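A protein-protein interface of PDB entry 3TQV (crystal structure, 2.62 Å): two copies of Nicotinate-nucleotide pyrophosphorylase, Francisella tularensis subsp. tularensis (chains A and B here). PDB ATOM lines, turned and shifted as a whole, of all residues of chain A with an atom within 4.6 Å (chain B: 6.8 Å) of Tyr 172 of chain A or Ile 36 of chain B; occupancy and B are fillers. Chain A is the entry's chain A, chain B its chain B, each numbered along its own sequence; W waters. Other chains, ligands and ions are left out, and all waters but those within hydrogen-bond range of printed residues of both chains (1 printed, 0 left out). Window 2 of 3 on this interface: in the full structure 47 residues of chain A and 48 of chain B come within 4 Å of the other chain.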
ATOM      1  N   ARG A 165     -24.067  -2.486  -2.717  1.00  0.00           N
ATOM      2  CA  ARG A 165     -23.548  -1.133  -2.576  1.00  0.00           C
ATOM      3  C   ARG A 165     -22.711  -0.762  -3.795  1.00  0.00           C
ATOM      4  O   ARG A 165     -22.140  -1.635  -4.435  1.00  0.00           O
ATOM      5  CB  ARG A 165     -22.736  -0.995  -1.295  1.00  0.00           C
ATOM      6  CG  ARG A 165     -21.352  -1.560  -1.395  1.00  0.00           C
ATOM      7  CD  ARG A 165     -20.627  -1.583  -0.046  1.00  0.00           C
ATOM      8  NE  ARG A 165     -19.462  -2.465  -0.129  1.00  0.00           N
ATOM      9  CZ  ARG A 165     -18.379  -2.387   0.631  1.00  0.00           C
ATOM     10  NH1 ARG A 165     -18.277  -1.466   1.578  1.00  0.00           N
ATOM     11  NH2 ARG A 165     -17.392  -3.245   0.423  1.00  0.00           N
ATOM     12  N   LEU A 168     -17.137   1.832  -1.741  1.00  0.00           N
ATOM     13  CA  LEU A 168     -16.702   1.766  -0.351  1.00  0.00           C
ATOM     14  C   LEU A 168     -17.290   2.919   0.450  1.00  0.00           C
ATOM     15  O   LEU A 168     -17.207   2.925   1.678  1.00  0.00           O
ATOM     16  CB  LEU A 168     -15.170   1.783  -0.252  1.00  0.00           C
ATOM     17  CG  LEU A 168     -14.404   0.607  -0.888  1.00  0.00           C
ATOM     18  CD1 LEU A 168     -12.895   0.850  -0.892  1.00  0.00           C
ATOM     19  CD2 LEU A 168     -14.737  -0.730  -0.227  1.00  0.00           C
ATOM     20  N   PHE A 169     -17.907   3.879  -0.244  1.00  0.00           N
ATOM     21  CA  PHE A 169     -18.458   5.083   0.404  1.00  0.00           C
ATOM     22  C   PHE A 169     -19.937   5.010   0.843  1.00  0.00           C
ATOM     23  O   PHE A 169     -20.336   5.702   1.777  1.00  0.00           O
ATOM     24  CB  PHE A 169     -18.276   6.288  -0.516  1.00  0.00           C
ATOM     25  CG  PHE A 169     -18.883   6.096  -1.879  1.00  0.00           C
ATOM     26  CD1 PHE A 169     -20.188   6.512  -2.142  1.00  0.00           C
ATOM     27  CD2 PHE A 169     -18.159   5.474  -2.895  1.00  0.00           C
ATOM     28  CE1 PHE A 169     -20.754   6.319  -3.398  1.00  0.00           C
ATOM     29  CE2 PHE A 169     -18.712   5.282  -4.162  1.00  0.00           C
ATOM     30  CZ  PHE A 169     -20.002   5.696  -4.413  1.00  0.00           C
ATOM     31  N   ALA A 171     -22.070   2.280   1.783  1.00  0.00           N
ATOM     32  CA  ALA A 171     -22.565   1.298   2.750  1.00  0.00           C
ATOM     33  C   ALA A 171     -21.403   0.645   3.475  1.00  0.00           C
ATOM     34  O   ALA A 171     -20.300   0.611   2.957  1.00  0.00           O
ATOM     35  CB  ALA A 171     -23.398   0.241   2.055  1.00  0.00           C
ATOM     36  N   TYR A 172     -21.656   0.125   4.670  1.00  0.00           N
ATOM     37  CA  TYR A 172     -20.631  -0.591   5.416  1.00  0.00           C
ATOM     38  C   TYR A 172     -20.532  -2.033   4.958  1.00  0.00           C
ATOM     39  O   TYR A 172     -21.532  -2.654   4.620  1.00  0.00           O
ATOM     40  CB  TYR A 172     -20.927  -0.570   6.920  1.00  0.00           C
ATOM     41  CG  TYR A 172     -20.548   0.723   7.602  1.00  0.00           C
ATOM     42  CD1 TYR A 172     -19.212   1.068   7.776  1.00  0.00           C
ATOM     43  CD2 TYR A 172     -21.525   1.605   8.079  1.00  0.00           C
ATOM     44  CE1 TYR A 172     -18.854   2.251   8.398  1.00  0.00           C
ATOM     45  CE2 TYR A 172     -21.175   2.795   8.706  1.00  0.00           C
ATOM     46  CZ  TYR A 172     -19.834   3.109   8.860  1.00  0.00           C
ATOM     47  OH  TYR A 172     -19.458   4.278   9.485  1.00  0.00           O
ATOM     48  N   LEU A 173     -19.319  -2.568   4.946  1.00  0.00           N
ATOM     49  CA  LEU A 173     -19.141  -4.006   4.748  1.00  0.00           C
ATOM     50  C   LEU A 173     -18.044  -4.540   5.647  1.00  0.00           C
ATOM     51  O   LEU A 173     -16.880  -4.588   5.265  1.00  0.00           O
ATOM     52  CB  LEU A 173     -18.878  -4.370   3.277  1.00  0.00           C
ATOM     53  CG  LEU A 173     -18.837  -5.882   3.001  1.00  0.00           C
ATOM     54  CD1 LEU A 173     -19.681  -6.666   4.013  1.00  0.00           C
ATOM     55  CD2 LEU A 173     -19.268  -6.200   1.584  1.00  0.00           C
ATOM     56  N   ILE A 174     -18.433  -4.934   6.853  1.00  0.00           N
ATOM     57  CA  ILE A 174     -17.480  -5.430   7.827  1.00  0.00           C
ATOM     58  C   ILE A 174     -17.065  -6.843   7.471  1.00  0.00           C
ATOM     59  O   ILE A 174     -17.857  -7.771   7.597  1.00  0.00           O
ATOM     60  CB  ILE A 174     -18.032  -5.385   9.257  1.00  0.00           C
ATOM     61  CG1 ILE A 174     -18.770  -4.064   9.491  1.00  0.00           C
ATOM     62  CG2 ILE A 174     -16.883  -5.532  10.240  1.00  0.00           C
ATOM     63  CD1 ILE A 174     -19.309  -3.894  10.884  1.00  0.00           C
ATOM     64  N   ALA A 192     -19.472   1.540  13.818  1.00  0.00           N
ATOM     65  CA  ALA A 192     -19.984   1.959  12.514  1.00  0.00           C
ATOM     66  C   ALA A 192     -21.200   2.872  12.646  1.00  0.00           C
ATOM     67  O   ALA A 192     -21.265   3.928  12.009  1.00  0.00           O
ATOM     68  CB  ALA A 192     -20.309   0.746  11.632  1.00  0.00           C
ATOM     69  N   LEU A 195     -20.072   6.343  13.919  1.00  0.00           N
ATOM     70  CA  LEU A 195     -19.537   7.146  12.845  1.00  0.00           C
ATOM     71  C   LEU A 195     -20.638   7.599  11.887  1.00  0.00           C
ATOM     72  O   LEU A 195     -20.516   8.644  11.249  1.00  0.00           O
ATOM     73  CB  LEU A 195     -18.481   6.340  12.086  1.00  0.00           C
ATOM     74  CG  LEU A 195     -17.062   6.235  12.650  1.00  0.00           C
ATOM     75  CD1 LEU A 195     -16.987   6.694  14.100  1.00  0.00           C
ATOM     76  CD2 LEU A 195     -16.529   4.820  12.495  1.00  0.00           C
ATOM     77  N   ASP A 196     -21.711   6.817  11.781  1.00  0.00           N
ATOM     78  CA  ASP A 196     -22.730   7.097  10.771  1.00  0.00           C
ATOM     79  C   ASP A 196     -23.928   6.146  10.879  1.00  0.00           C
ATOM     80  O   ASP A 196     -23.930   5.064  10.288  1.00  0.00           O
ATOM     81  CB  ASP A 196     -22.102   7.019   9.371  1.00  0.00           C
ATOM     82  CG  ASP A 196     -22.885   7.794   8.319  1.00  0.00           C
ATOM     83  OD1 ASP A 196     -22.280   8.147   7.284  1.00  0.00           O
ATOM     84  OD2 ASP A 196     -24.096   8.050   8.517  1.00  0.00           O
ATOM     85  N   LYS A 199     -26.114   4.626   7.445  1.00  0.00           N
ATOM     86  CA  LYS A 199     -25.729   3.681   6.396  1.00  0.00           C
ATOM     87  C   LYS A 199     -26.118   2.264   6.732  1.00  0.00           C
ATOM     88  O   LYS A 199     -26.233   1.890   7.901  1.00  0.00           O
ATOM     89  CB  LYS A 199     -24.222   3.706   6.137  1.00  0.00           C
ATOM     90  CG  LYS A 199     -23.640   5.082   6.019  1.00  0.00           C
ATOM     91  CD  LYS A 199     -23.594   5.589   4.589  1.00  0.00           C
ATOM     92  CE  LYS A 199     -23.346   7.089   4.616  1.00  0.00           C
ATOM     93  NZ  LYS A 199     -22.714   7.591   3.387  1.00  0.00           N
ATOM     94  N   VAL A 200     -26.301   1.471   5.685  1.00  0.00           N
ATOM     95  CA  VAL A 200     -26.456   0.043   5.836  1.00  0.00           C
ATOM     96  C   VAL A 200     -25.184  -0.483   6.480  1.00  0.00           C
ATOM     97  O   VAL A 200     -24.076  -0.137   6.056  1.00  0.00           O
ATOM     98  CB  VAL A 200     -26.665  -0.628   4.468  1.00  0.00           C
ATOM     99  CG1 VAL A 200     -26.647  -2.149   4.585  1.00  0.00           C
ATOM    100  CG2 VAL A 200     -27.965  -0.138   3.842  1.00  0.00           C
ATOM    101  N   VAL A 201     -25.338  -1.293   7.522  1.00  0.00           N
ATOM    102  CA  VAL A 201     -24.214  -2.033   8.065  1.00  0.00           C
ATOM    103  C   VAL A 201     -24.314  -3.485   7.632  1.00  0.00           C
ATOM    104  O   VAL A 201     -25.231  -4.195   8.023  1.00  0.00           O
ATOM    105  CB  VAL A 201     -24.189  -1.985   9.596  1.00  0.00           C
ATOM    106  CG1 VAL A 201     -23.013  -2.795  10.122  1.00  0.00           C
ATOM    107  CG2 VAL A 201     -24.128  -0.549  10.089  1.00  0.00           C
ATOM    108  N   GLU A 202     -23.387  -3.935   6.807  1.00  0.00           N
ATOM    109  CA  GLU A 202     -23.349  -5.350   6.478  1.00  0.00           C
ATOM    110  C   GLU A 202     -22.123  -6.000   7.130  1.00  0.00           C
ATOM    111  O   GLU A 202     -21.081  -5.371   7.289  1.00  0.00           O
ATOM    112  CB  GLU A 202     -23.354  -5.567   4.961  1.00  0.00           C
ATOM    113  CG  GLU A 202     -23.263  -7.034   4.564  1.00  0.00           C
ATOM    114  CD  GLU A 202     -23.542  -7.285   3.085  1.00  0.00           C
ATOM    115  OE1 GLU A 202     -23.362  -6.348   2.266  1.00  0.00           O
ATOM    116  OE2 GLU A 202     -23.954  -8.423   2.755  1.00  0.00           O
ATOM    117  N   ILE B  31     -14.281   4.974  -4.592  1.00  0.00           N
ATOM    118  CA  ILE B  31     -13.947   5.550  -3.287  1.00  0.00           C
ATOM    119  C   ILE B  31     -14.709   6.832  -2.947  1.00  0.00           C
ATOM    120  O   ILE B  31     -15.128   7.042  -1.798  1.00  0.00           O
ATOM    121  CB  ILE B  31     -12.432   5.818  -3.168  1.00  0.00           C
ATOM    122  CG1 ILE B  31     -11.673   4.483  -3.097  1.00  0.00           C
ATOM    123  CG2 ILE B  31     -12.130   6.726  -1.965  1.00  0.00           C
ATOM    124  CD1 ILE B  31     -10.167   4.603  -3.315  1.00  0.00           C
ATOM    125  N   THR B  33     -15.930   9.931  -1.502  1.00  0.00           N
ATOM    126  CA  THR B  33     -15.526  10.708  -0.335  1.00  0.00           C
ATOM    127  C   THR B  33     -14.682   9.942   0.670  1.00  0.00           C
ATOM    128  O   THR B  33     -14.019  10.550   1.511  1.00  0.00           O
ATOM    129  CB  THR B  33     -16.735  11.320   0.396  1.00  0.00           C
ATOM    130  OG1 THR B  33     -17.674  10.287   0.731  1.00  0.00           O
ATOM    131  CG2 THR B  33     -17.397  12.396  -0.478  1.00  0.00           C
ATOM    132  N   GLY B  34     -14.703   8.616   0.605  1.00  0.00           N
ATOM    133  CA  GLY B  34     -13.830   7.833   1.453  1.00  0.00           C
ATOM    134  C   GLY B  34     -14.355   6.463   1.811  1.00  0.00           C
ATOM    135  O   GLY B  34     -15.561   6.270   2.014  1.00  0.00           O
ATOM    136  N   ASP B  35     -13.436   5.505   1.882  1.00  0.00           N
ATOM    137  CA  ASP B  35     -13.745   4.157   2.339  1.00  0.00           C
ATOM    138  C   ASP B  35     -14.206   4.213   3.791  1.00  0.00           C
ATOM    139  O   ASP B  35     -13.389   4.334   4.711  1.00  0.00           O
ATOM    140  CB  ASP B  35     -12.497   3.289   2.214  1.00  0.00           C
ATOM    141  CG  ASP B  35     -12.762   1.831   2.517  1.00  0.00           C
ATOM    142  OD1 ASP B  35     -13.815   1.512   3.124  1.00  0.00           O
ATOM    143  OD2 ASP B  35     -11.897   1.006   2.145  1.00  0.00           O
ATOM    144  N   ILE B  36     -15.511   4.141   4.011  1.00  0.00           N
ATOM    145  CA  ILE B  36     -16.025   4.327   5.367  1.00  0.00           C
ATOM    146  C   ILE B  36     -15.732   3.164   6.298  1.00  0.00           C
ATOM    147  O   ILE B  36     -15.578   3.365   7.498  1.00  0.00           O
ATOM    148  CB  ILE B  36     -17.543   4.642   5.411  1.00  0.00           C
ATOM    149  CG1 ILE B  36     -18.372   3.476   4.867  1.00  0.00           C
ATOM    150  CG2 ILE B  36     -17.851   5.945   4.683  1.00  0.00           C
ATOM    151  CD1 ILE B  36     -19.881   3.696   4.988  1.00  0.00           C
ATOM    152  N   THR B  37     -15.661   1.955   5.749  1.00  0.00           N
ATOM    153  CA  THR B  37     -15.461   0.756   6.560  1.00  0.00           C
ATOM    154  C   THR B  37     -13.993   0.595   6.945  1.00  0.00           C
ATOM    155  O   THR B  37     -13.671   0.022   7.988  1.00  0.00           O
ATOM    156  CB  THR B  37     -15.967  -0.517   5.842  1.00  0.00           C
ATOM    157  OG1 THR B  37     -17.357  -0.377   5.539  1.00  0.00           O
ATOM    158  CG2 THR B  37     -15.794  -1.730   6.721  1.00  0.00           C
ATOM    159  N   ALA B  38     -13.102   1.107   6.105  1.00  0.00           N
ATOM    160  CA  ALA B  38     -11.677   1.106   6.421  1.00  0.00           C
ATOM    161  C   ALA B  38     -11.400   1.886   7.710  1.00  0.00           C
ATOM    162  O   ALA B  38     -10.415   1.637   8.407  1.00  0.00           O
ATOM    163  CB  ALA B  38     -10.875   1.682   5.263  1.00  0.00           C
ATOM    164  N   GLN B  39     -12.289   2.817   8.024  1.00  0.00           N
ATOM    165  CA  GLN B  39     -12.126   3.674   9.184  1.00  0.00           C
ATOM    166  C   GLN B  39     -12.283   2.903  10.478  1.00  0.00           C
ATOM    167  O   GLN B  39     -11.964   3.408  11.560  1.00  0.00           O
ATOM    168  CB  GLN B  39     -13.121   4.825   9.124  1.00  0.00           C
ATOM    169  CG  GLN B  39     -12.725   5.875   8.107  1.00  0.00           C
ATOM    170  CD  GLN B  39     -11.352   6.443   8.402  1.00  0.00           C
ATOM    171  OE1 GLN B  39     -11.018   6.707   9.561  1.00  0.00           O
ATOM    172  NE2 GLN B  39     -10.539   6.613   7.362  1.00  0.00           N
ATOM    173  N   LEU B  40     -12.774   1.673  10.357  1.00  0.00           N
ATOM    174  CA  LEU B  40     -12.977   0.814  11.511  1.00  0.00           C
ATOM    175  C   LEU B  40     -11.743  -0.033  11.807  1.00  0.00           C
ATOM    176  O   LEU B  40     -11.713  -0.758  12.803  1.00  0.00           O
ATOM    177  CB  LEU B  40     -14.208  -0.075  11.311  1.00  0.00           C
ATOM    178  CG  LEU B  40     -15.576   0.603  11.121  1.00  0.00           C
ATOM    179  CD1 LEU B  40     -16.597  -0.387  10.610  1.00  0.00           C
ATOM    180  CD2 LEU B  40     -16.082   1.258  12.403  1.00  0.00           C
HETATM  181  O   HOH W   1     -16.690   0.306   3.155  1.00  0.00           O
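The backbone carbonyl oxygen (O) of Leu 168 of chain A sits at hydrogen-bond distance from the backbone NH (N) of Ile 36 of chain B.
The backbone NH of Leu 173 of chain A sits at hydrogen-bond distance from the side-chain hydroxyl of Thr 37 of chain B (3.0 Å).
O of Ala 171 of chain A lies within hydrogen-bond range of NH1 of Arg 165 of chain A, 3.2 Å away.
The backbone carbonyl oxygen of Ala 192 of chain A lies within hydrogen-bond range of the side-chain hydroxyl of Tyr 172 of chain A, 3.1 Å away.
The backbone carbonyl oxygen (O) of Val 200 of chain A lies within hydrogen-bond range of the backbone NH (N) of Tyr 172 of chain A (2.8 Å).
O of Tyr 172 of chain A lies within hydrogen-bond range of N of Glu 202 of chain A (3.1 Å).
N of Thr 37 of chain B sits at hydrogen-bond distance from OD1 of Asp 35 of chain B (3.2 Å).
The side-chain carboxylate of Asp 35 of chain B lies within hydrogen-bond range of the backbone NH of Ala 38 of chain B (3.1 Å).
Gly 34 of chain B touches Leu 168 of chain A.
Leu 168 of chain A touches Asp 35 of chain B (CD1 to OD2, 3.2 Å).
O of Ile 31 of chain B touches CB of Phe 169 of chain A, at 3.5 Å.
CA of Phe 169 of chain A touches O of Gly 34 of chain B, at 3.5 Å.
Ile 36 of chain B touches Phe 169 of chain A.
O of Ala 171 of chain A touches CD1 of Ile 36 of chain B, at 3.7 Å.
Tyr 172 of chain A touches Ile 36 of chain B (CE1 to O, 3.6 Å).
Tyr 172 of chain A touches Thr 37 of chain B (CD1 to OG1, 3.2 Å).
Ala 192 of chain A touches Leu 40 of chain B (N to CD2, 3.7 Å).
Leu 40 of chain B touches Leu 195 of chain A.
Arg 165 of chain A touches none of the printed residues of chain B.
Of chain B, only Ile 36 (3.6 Å) and Thr 37 (3.2 Å) come within 4 Å of Tyr 172 of chain A.
Of the printed residues of chain B, Leu 173 of chain A touches Thr 37.
Of the printed residues of chain A, Ile 31 of chain B touches Phe 169 (3.5 Å).
Ile 36 of chain B touches four residues of chain A.
Of the printed residues of chain A, Leu 40 of chain B touches Ala 192 (3.7 Å) and Leu 195 (3.6 Å).
Of the 9 printed residues of chain B, 6 touch a printed residue of chain A.
Along chain B the printed residues that touch a printed residue of chain A span positions 31 to 40.
Along chain A the printed residues that touch a printed residue of chain B span positions 168 to 195.
Among the printed residues, 12 pairs touch across the chains.
Among the printed residues, no Asp or Glu carboxylate lies within 4 Å of a Lys or Arg side-chain nitrogen of the other chain.
No position is printed for both chains.
Water W1 lies within hydrogen-bond range of OG1 of Thr 37 of chain B (2.6 Å), NH1 of Arg 165 of chain A (2.9 Å), O of Leu 168 of chain A (3.1 Å) and OD1 of Asp 35 of chain B (3.1 Å).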
